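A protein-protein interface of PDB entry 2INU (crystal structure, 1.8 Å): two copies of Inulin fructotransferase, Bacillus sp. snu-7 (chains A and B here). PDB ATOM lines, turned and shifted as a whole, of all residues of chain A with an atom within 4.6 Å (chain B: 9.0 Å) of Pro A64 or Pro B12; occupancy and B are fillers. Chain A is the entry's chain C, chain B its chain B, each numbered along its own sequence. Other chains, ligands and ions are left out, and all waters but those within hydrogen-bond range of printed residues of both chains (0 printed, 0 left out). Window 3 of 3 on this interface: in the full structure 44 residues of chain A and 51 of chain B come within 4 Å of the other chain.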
ATOM      1  N   THR A  18     -22.438 -31.457  18.525  1.00  0.00           N
ATOM      2  CA  THR A  18     -21.105 -32.063  18.492  1.00  0.00           C
ATOM      3  C   THR A  18     -20.549 -32.651  19.803  1.00  0.00           C
ATOM      4  O   THR A  18     -19.641 -33.481  19.758  1.00  0.00           O
ATOM      5  CB  THR A  18     -20.043 -31.072  17.943  1.00  0.00           C
ATOM      6  OG1 THR A  18     -19.850 -30.001  18.879  1.00  0.00           O
ATOM      7  CG2 THR A  18     -20.493 -30.489  16.605  1.00  0.00           C
ATOM      8  N   ILE A  62     -26.460 -26.221  16.462  1.00  0.00           N
ATOM      9  CA  ILE A  62     -25.695 -26.957  15.465  1.00  0.00           C
ATOM     10  C   ILE A  62     -24.506 -26.120  14.980  1.00  0.00           C
ATOM     11  O   ILE A  62     -24.658 -25.227  14.143  1.00  0.00           O
ATOM     12  CB  ILE A  62     -26.567 -27.346  14.256  1.00  0.00           C
ATOM     13  CG1 ILE A  62     -27.740 -28.208  14.723  1.00  0.00           C
ATOM     14  CG2 ILE A  62     -25.731 -28.134  13.243  1.00  0.00           C
ATOM     15  CD1 ILE A  62     -28.855 -28.353  13.702  1.00  0.00           C
ATOM     16  N   PRO A  63     -23.312 -26.385  15.528  1.00  0.00           N
ATOM     17  CA  PRO A  63     -22.043 -25.716  15.209  1.00  0.00           C
ATOM     18  C   PRO A  63     -21.702 -25.678  13.713  1.00  0.00           C
ATOM     19  O   PRO A  63     -22.188 -26.498  12.933  1.00  0.00           O
ATOM     20  CB  PRO A  63     -21.031 -26.540  15.990  1.00  0.00           C
ATOM     21  CG  PRO A  63     -21.770 -26.827  17.243  1.00  0.00           C
ATOM     22  CD  PRO A  63     -23.178 -27.183  16.765  1.00  0.00           C
ATOM     23  N   PRO A  64     -20.899 -24.689  13.288  1.00  0.00           N
ATOM     24  CA  PRO A  64     -20.529 -24.625  11.875  1.00  0.00           C
ATOM     25  C   PRO A  64     -19.932 -25.967  11.467  1.00  0.00           C
ATOM     26  O   PRO A  64     -19.008 -26.448  12.099  1.00  0.00           O
ATOM     27  CB  PRO A  64     -19.492 -23.502  11.847  1.00  0.00           C
ATOM     28  CG  PRO A  64     -20.053 -22.553  12.842  1.00  0.00           C
ATOM     29  CD  PRO A  64     -20.545 -23.438  13.983  1.00  0.00           C
ATOM     30  N   GLY A  65     -20.443 -26.565  10.400  1.00  0.00           N
ATOM     31  CA  GLY A  65     -19.898 -27.837   9.972  1.00  0.00           C
ATOM     32  C   GLY A  65     -20.680 -28.635   8.961  1.00  0.00           C
ATOM     33  O   GLY A  65     -21.769 -28.261   8.543  1.00  0.00           O
ATOM     34  N   TYR A  67     -22.555 -32.079   8.304  1.00  0.00           N
ATOM     35  CA  TYR A  67     -23.206 -33.185   9.008  1.00  0.00           C
ATOM     36  C   TYR A  67     -24.124 -34.000   8.093  1.00  0.00           C
ATOM     37  O   TYR A  67     -24.914 -33.441   7.332  1.00  0.00           O
ATOM     38  CB  TYR A  67     -24.049 -32.655  10.174  1.00  0.00           C
ATOM     39  CG  TYR A  67     -23.326 -31.683  11.070  1.00  0.00           C
ATOM     40  CD1 TYR A  67     -22.420 -32.130  12.029  1.00  0.00           C
ATOM     41  CD2 TYR A  67     -23.538 -30.312  10.948  1.00  0.00           C
ATOM     42  CE1 TYR A  67     -21.746 -31.230  12.851  1.00  0.00           C
ATOM     43  CE2 TYR A  67     -22.870 -29.406  11.764  1.00  0.00           C
ATOM     44  CZ  TYR A  67     -21.976 -29.869  12.708  1.00  0.00           C
ATOM     45  OH  TYR A  67     -21.309 -28.973  13.508  1.00  0.00           O
ATOM     46  N   PHE A  85     -25.591 -21.361  12.999  1.00  0.00           N
ATOM     47  CA  PHE A  85     -24.954 -20.057  12.876  1.00  0.00           C
ATOM     48  C   PHE A  85     -25.009 -19.502  11.452  1.00  0.00           C
ATOM     49  O   PHE A  85     -24.432 -18.437  11.185  1.00  0.00           O
ATOM     50  CB  PHE A  85     -23.482 -20.112  13.312  1.00  0.00           C
ATOM     51  CG  PHE A  85     -23.278 -20.446  14.749  1.00  0.00           C
ATOM     52  CD1 PHE A  85     -23.362 -21.762  15.191  1.00  0.00           C
ATOM     53  CD2 PHE A  85     -22.984 -19.445  15.668  1.00  0.00           C
ATOM     54  CE1 PHE A  85     -23.154 -22.070  16.537  1.00  0.00           C
ATOM     55  CE2 PHE A  85     -22.776 -19.749  17.009  1.00  0.00           C
ATOM     56  CZ  PHE A  85     -22.861 -21.056  17.438  1.00  0.00           C
ATOM     57  N   ALA A 110     -21.908 -23.259   6.513  1.00  0.00           N
ATOM     58  CA  ALA A 110     -22.507 -22.856   7.788  1.00  0.00           C
ATOM     59  C   ALA A 110     -22.858 -24.143   8.532  1.00  0.00           C
ATOM     60  O   ALA A 110     -22.096 -25.113   8.477  1.00  0.00           O
ATOM     61  CB  ALA A 110     -23.766 -22.012   7.556  1.00  0.00           C
ATOM     62  N   SER A 111     -23.995 -24.158   9.226  1.00  0.00           N
ATOM     63  CA  SER A 111     -24.427 -25.356   9.942  1.00  0.00           C
ATOM     64  C   SER A 111     -25.171 -26.169   8.886  1.00  0.00           C
ATOM     65  O   SER A 111     -26.409 -26.165   8.800  1.00  0.00           O
ATOM     66  CB  SER A 111     -25.335 -24.967  11.103  1.00  0.00           C
ATOM     67  OG  SER A 111     -24.683 -23.977  11.888  1.00  0.00           O
ATOM     68  N   PRO B  12     -16.964 -26.549  17.992  1.00  0.00           N
ATOM     69  CA  PRO B  12     -16.280 -26.654  16.689  1.00  0.00           C
ATOM     70  C   PRO B  12     -16.571 -25.521  15.704  1.00  0.00           C
ATOM     71  O   PRO B  12     -17.720 -25.113  15.517  1.00  0.00           O
ATOM     72  CB  PRO B  12     -16.672 -28.004  16.130  1.00  0.00           C
ATOM     73  CG  PRO B  12     -16.687 -28.829  17.420  1.00  0.00           C
ATOM     74  CD  PRO B  12     -17.238 -27.898  18.523  1.00  0.00           C
ATOM     75  N   ASN B  13     -15.500 -25.023  15.089  1.00  0.00           N
ATOM     76  CA  ASN B  13     -15.576 -23.934  14.124  1.00  0.00           C
ATOM     77  C   ASN B  13     -16.210 -22.688  14.726  1.00  0.00           C
ATOM     78  O   ASN B  13     -16.709 -21.815  14.002  1.00  0.00           O
ATOM     79  CB  ASN B  13     -16.366 -24.369  12.893  1.00  0.00           C
ATOM     80  CG  ASN B  13     -15.633 -25.429  12.074  1.00  0.00           C
ATOM     81  OD1 ASN B  13     -16.253 -26.302  11.479  1.00  0.00           O
ATOM     82  ND2 ASN B  13     -14.306 -25.356  12.049  1.00  0.00           N
ATOM     83  N   THR B  14     -16.187 -22.599  16.052  1.00  0.00           N
ATOM     84  CA  THR B  14     -16.754 -21.445  16.743  1.00  0.00           C
ATOM     85  C   THR B  14     -15.627 -20.788  17.532  1.00  0.00           C
ATOM     86  O   THR B  14     -14.934 -21.458  18.307  1.00  0.00           O
ATOM     87  CB  THR B  14     -17.865 -21.859  17.743  1.00  0.00           C
ATOM     88  OG1 THR B  14     -18.850 -22.654  17.075  1.00  0.00           O
ATOM     89  CG2 THR B  14     -18.546 -20.630  18.329  1.00  0.00           C
ATOM     90  N   TYR B  15     -15.423 -19.490  17.319  1.00  0.00           N
ATOM     91  CA  TYR B  15     -14.380 -18.765  18.048  1.00  0.00           C
ATOM     92  C   TYR B  15     -15.031 -17.586  18.772  1.00  0.00           C
ATOM     93  O   TYR B  15     -16.101 -17.113  18.386  1.00  0.00           O
ATOM     94  CB  TYR B  15     -13.311 -18.181  17.112  1.00  0.00           C
ATOM     95  CG  TYR B  15     -12.646 -19.138  16.132  1.00  0.00           C
ATOM     96  CD1 TYR B  15     -13.341 -19.658  15.040  1.00  0.00           C
ATOM     97  CD2 TYR B  15     -11.296 -19.460  16.260  1.00  0.00           C
ATOM     98  CE1 TYR B  15     -12.718 -20.464  14.104  1.00  0.00           C
ATOM     99  CE2 TYR B  15     -10.650 -20.271  15.316  1.00  0.00           C
ATOM    100  CZ  TYR B  15     -11.367 -20.768  14.242  1.00  0.00           C
ATOM    101  OH  TYR B  15     -10.749 -21.564  13.304  1.00  0.00           O
ATOM    102  N   ILE B  45      -8.781 -21.022  10.141  1.00  0.00           N
ATOM    103  CA  ILE B  45      -9.891 -21.681   9.470  1.00  0.00           C
ATOM    104  C   ILE B  45      -9.365 -22.270   8.167  1.00  0.00           C
ATOM    105  O   ILE B  45      -9.630 -23.440   7.855  1.00  0.00           O
ATOM    106  CB  ILE B  45     -11.016 -20.681   9.150  1.00  0.00           C
ATOM    107  CG1 ILE B  45     -11.606 -20.138  10.450  1.00  0.00           C
ATOM    108  CG2 ILE B  45     -12.100 -21.356   8.313  1.00  0.00           C
ATOM    109  CD1 ILE B  45     -12.600 -19.007  10.251  1.00  0.00           C
ATOM    110  N   ARG B  48      -7.190 -25.266   8.699  1.00  0.00           N
ATOM    111  CA  ARG B  48      -7.964 -26.476   8.870  1.00  0.00           C
ATOM    112  C   ARG B  48      -8.816 -26.954   7.695  1.00  0.00           C
ATOM    113  O   ARG B  48      -8.762 -28.131   7.342  1.00  0.00           O
ATOM    114  CB  ARG B  48      -8.809 -26.304  10.133  1.00  0.00           C
ATOM    115  CG  ARG B  48      -7.917 -26.104  11.364  1.00  0.00           C
ATOM    116  CD  ARG B  48      -8.685 -25.949  12.678  1.00  0.00           C
ATOM    117  NE  ARG B  48      -9.669 -24.876  12.616  1.00  0.00           N
ATOM    118  CZ  ARG B  48     -10.944 -25.062  12.288  1.00  0.00           C
ATOM    119  NH1 ARG B  48     -11.382 -26.281  12.001  1.00  0.00           N
ATOM    120  NH2 ARG B  48     -11.779 -24.034  12.245  1.00  0.00           N
ATOM    121  N   GLN B  49      -9.592 -26.069   7.078  1.00  0.00           N
ATOM    122  CA  GLN B  49     -10.438 -26.485   5.962  1.00  0.00           C
ATOM    123  C   GLN B  49      -9.740 -26.248   4.627  1.00  0.00           C
ATOM    124  O   GLN B  49      -9.913 -25.213   3.980  1.00  0.00           O
ATOM    125  CB  GLN B  49     -11.771 -25.742   6.040  1.00  0.00           C
ATOM    126  CG  GLN B  49     -12.355 -25.794   7.450  1.00  0.00           C
ATOM    127  CD  GLN B  49     -13.641 -25.023   7.626  1.00  0.00           C
ATOM    128  OE1 GLN B  49     -14.205 -24.994   8.727  1.00  0.00           O
ATOM    129  NE2 GLN B  49     -14.132 -24.416   6.545  1.00  0.00           N
ATOM    130  N   ARG B  55     -15.376 -27.230   3.351  1.00  0.00           N
ATOM    131  CA  ARG B  55     -15.143 -25.863   3.803  1.00  0.00           C
ATOM    132  C   ARG B  55     -16.436 -25.195   4.273  1.00  0.00           C
ATOM    133  O   ARG B  55     -16.978 -24.290   3.623  1.00  0.00           O
ATOM    134  CB  ARG B  55     -14.407 -25.050   2.732  1.00  0.00           C
ATOM    135  CG  ARG B  55     -12.945 -25.494   2.660  1.00  0.00           C
ATOM    136  CD  ARG B  55     -11.986 -24.446   2.102  1.00  0.00           C
ATOM    137  NE  ARG B  55     -11.925 -24.454   0.648  1.00  0.00           N
ATOM    138  CZ  ARG B  55     -10.808 -24.298  -0.054  1.00  0.00           C
ATOM    139  NH1 ARG B  55      -9.652 -24.123   0.561  1.00  0.00           N
ATOM    140  NH2 ARG B  55     -10.842 -24.327  -1.376  1.00  0.00           N
ATOM    141  N   PRO B  56     -16.971 -25.701   5.399  1.00  0.00           N
ATOM    142  CA  PRO B  56     -18.172 -25.343   6.162  1.00  0.00           C
ATOM    143  C   PRO B  56     -18.128 -23.895   6.609  1.00  0.00           C
ATOM    144  O   PRO B  56     -19.156 -23.225   6.711  1.00  0.00           O
ATOM    145  CB  PRO B  56     -18.098 -26.281   7.357  1.00  0.00           C
ATOM    146  CG  PRO B  56     -17.570 -27.516   6.750  1.00  0.00           C
ATOM    147  CD  PRO B  56     -16.465 -27.017   5.842  1.00  0.00           C
ATOM    148  N   GLY B  57     -16.921 -23.433   6.906  1.00  0.00           N
ATOM    149  CA  GLY B  57     -16.744 -22.072   7.359  1.00  0.00           C
ATOM    150  C   GLY B  57     -16.674 -22.085   8.864  1.00  0.00           C
ATOM    151  O   GLY B  57     -16.264 -23.081   9.460  1.00  0.00           O
ATOM    152  N   ALA B  58     -17.068 -20.985   9.487  1.00  0.00           N
ATOM    153  CA  ALA B  58     -17.036 -20.914  10.930  1.00  0.00           C
ATOM    154  C   ALA B  58     -17.765 -19.693  11.434  1.00  0.00           C
ATOM    155  O   ALA B  58     -18.257 -18.874  10.656  1.00  0.00           O
ATOM    156  CB  ALA B  58     -15.594 -20.897  11.412  1.00  0.00           C
ATOM    157  N   ALA B  59     -17.836 -19.594  12.753  1.00  0.00           N
ATOM    158  CA  ALA B  59     -18.486 -18.477  13.394  1.00  0.00           C
ATOM    159  C   ALA B  59     -17.500 -17.811  14.335  1.00  0.00           C
ATOM    160  O   ALA B  59     -16.780 -18.475  15.077  1.00  0.00           O
ATOM    161  CB  ALA B  59     -19.708 -18.955  14.162  1.00  0.00           C
ATOM    162  N   ILE B  60     -17.463 -16.486  14.271  1.00  0.00           N
ATOM    163  CA  ILE B  60     -16.605 -15.685  15.126  1.00  0.00           C
ATOM    164  C   ILE B  60     -17.537 -14.799  15.938  1.00  0.00           C
ATOM    165  O   ILE B  60     -18.228 -13.940  15.395  1.00  0.00           O
ATOM    166  CB  ILE B  60     -15.638 -14.818  14.292  1.00  0.00           C
ATOM    167  CG1 ILE B  60     -14.739 -15.718  13.435  1.00  0.00           C
ATOM    168  CG2 ILE B  60     -14.792 -13.944  15.208  1.00  0.00           C
ATOM    169  CD1 ILE B  60     -13.798 -14.965  12.522  1.00  0.00           C
ATOM    170  N   ILE B  61     -17.561 -15.045  17.242  1.00  0.00           N
ATOM    171  CA  ILE B  61     -18.413 -14.323  18.178  1.00  0.00           C
ATOM    172  C   ILE B  61     -17.696 -13.123  18.792  1.00  0.00           C
ATOM    173  O   ILE B  61     -16.548 -13.252  19.238  1.00  0.00           O
ATOM    174  CB  ILE B  61     -18.852 -15.248  19.330  1.00  0.00           C
ATOM    175  CG1 ILE B  61     -19.538 -16.490  18.767  1.00  0.00           C
ATOM    176  CG2 ILE B  61     -19.744 -14.491  20.295  1.00  0.00           C
ATOM    177  CD1 ILE B  61     -20.685 -16.204  17.824  1.00  0.00           C
ATOM    178  N   SER B  78     -16.042 -18.571   2.433  1.00  0.00           N
ATOM    179  CA  SER B  78     -17.467 -18.640   2.302  1.00  0.00           C
ATOM    180  C   SER B  78     -18.095 -19.120   3.581  1.00  0.00           C
ATOM    181  O   SER B  78     -17.474 -19.831   4.375  1.00  0.00           O
ATOM    182  CB  SER B  78     -17.854 -19.578   1.164  1.00  0.00           C
ATOM    183  OG  SER B  78     -17.634 -18.967  -0.101  1.00  0.00           O
ATOM    184  N   TYR B  79     -19.341 -18.705   3.769  1.00  0.00           N
ATOM    185  CA  TYR B  79     -20.122 -19.095   4.933  1.00  0.00           C
ATOM    186  C   TYR B  79     -19.459 -18.668   6.257  1.00  0.00           C
ATOM    187  O   TYR B  79     -19.512 -19.392   7.251  1.00  0.00           O
ATOM    188  CB  TYR B  79     -20.348 -20.617   4.921  1.00  0.00           C
ATOM    189  CG  TYR B  79     -20.486 -21.251   3.530  1.00  0.00           C
ATOM    190  CD1 TYR B  79     -21.589 -20.994   2.700  1.00  0.00           C
ATOM    191  CD2 TYR B  79     -19.509 -22.136   3.053  1.00  0.00           C
ATOM    192  CE1 TYR B  79     -21.718 -21.635   1.449  1.00  0.00           C
ATOM    193  CE2 TYR B  79     -19.639 -22.769   1.810  1.00  0.00           C
ATOM    194  CZ  TYR B  79     -20.738 -22.506   1.011  1.00  0.00           C
ATOM    195  OH  TYR B  79     -20.847 -23.138  -0.215  1.00  0.00           O
ATOM    196  N   LEU B  80     -18.837 -17.490   6.273  1.00  0.00           N
ATOM    197  CA  LEU B  80     -18.208 -16.970   7.493  1.00  0.00           C
ATOM    198  C   LEU B  80     -19.243 -16.106   8.196  1.00  0.00           C
ATOM    199  O   LEU B  80     -19.877 -15.251   7.576  1.00  0.00           O
ATOM    200  CB  LEU B  80     -16.979 -16.113   7.169  1.00  0.00           C
ATOM    201  CG  LEU B  80     -16.140 -15.826   8.314  1.00  0.00           C
ATOM    202  CD1 LEU B  80     -15.900 -17.048   9.468  1.00  0.00           C
ATOM    203  CD2 LEU B  80     -15.062 -14.833   8.167  1.00  0.00           C
ATOM    204  N   THR B  81     -19.427 -16.358   9.484  1.00  0.00           N
ATOM    205  CA  THR B  81     -20.381 -15.605  10.278  1.00  0.00           C
ATOM    206  C   THR B  81     -19.665 -14.862  11.393  1.00  0.00           C
ATOM    207  O   THR B  81     -18.982 -15.477  12.216  1.00  0.00           O
ATOM    208  CB  THR B  81     -21.437 -16.523  10.951  1.00  0.00           C
ATOM    209  OG1 THR B  81     -22.325 -17.061   9.962  1.00  0.00           O
ATOM    210  CG2 THR B  81     -22.238 -15.724  11.992  1.00  0.00           C
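ND2 of Asn B13 sits close to NH2 of Arg B48, 2.9 Å away.
ND2 of Asn B13 sits at hydrogen-bond distance from OE1 of Gln B49, 3.3 Å away.
The backbone carbonyl oxygen (O) of Ala A110 is in hydrogen-bond range of the backbone NH (N) of Gly A65.
The backbone NH (N) of Phe A85 sits at hydrogen-bond distance from the side-chain hydroxyl (OG) of Ser A111 (3.0 Å).
The backbone NH of Ile B60 is in hydrogen-bond range of the backbone carbonyl oxygen of Thr B81, 2.7 Å away.
N of Tyr B15 is in hydrogen-bond range of O of Ala B59 (2.8 Å).
Printed residues of chain B within 4 Å of Thr A18: Pro B12.
Pro A64 touches just these residues of chain B: Pro B12, Asn B13, Thr B14, Ala B58 and Ala B59.
Pro B12 touches just these residues of chain A: Thr A18, Pro A63 and Pro A64.
Printed residues of chain A within 4 Å of Ala B58: Pro A64.
Leu B80 touches none of the printed residues of chain A.
Printed residues of chain A within 4 Å of Thr B81: Phe A85.
The nearest printed residue of chain B that does not touch Phe A85 is Ile B61 (4.2 Å).
Among the printed residues, pairs that only touch across the chains: Thr A18 with Pro B12, Pro A63 with Pro B12, Pro A64 with Pro B12, Pro A64 with Thr B14, Pro A64 with Ala B58, Pro A64 with Ala B59, Gly A65 with Pro B56, Phe A85 with Ala B59 and Ala A110 with Tyr B79.
The backbone carbonyl oxygen of Phe A85 sits at hydrogen-bond distance from the side-chain hydroxyl of Thr B81.
O of Pro B56 lies within hydrogen-bond range of N of Ala A110, at 2.8 Å.
The side-chain amide oxygen (OD1) of Asn B13 lies close to the backbone carbonyl oxygen (O) of Pro A64 (2.8 Å).
No position is printed for both chains.
Along chain B the printed residues that touch a printed residue of chain A span positions 12 to 81.
Of the 9 printed residues of chain A, 6 touch a printed residue of chain B.
Along chain A the printed residues that touch a printed residue of chain B span positions 18 to 110.
Among the printed residues, no Asp or Glu carboxylate lies within 4 Å of a Lys or Arg side-chain nitrogen of the other chain.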
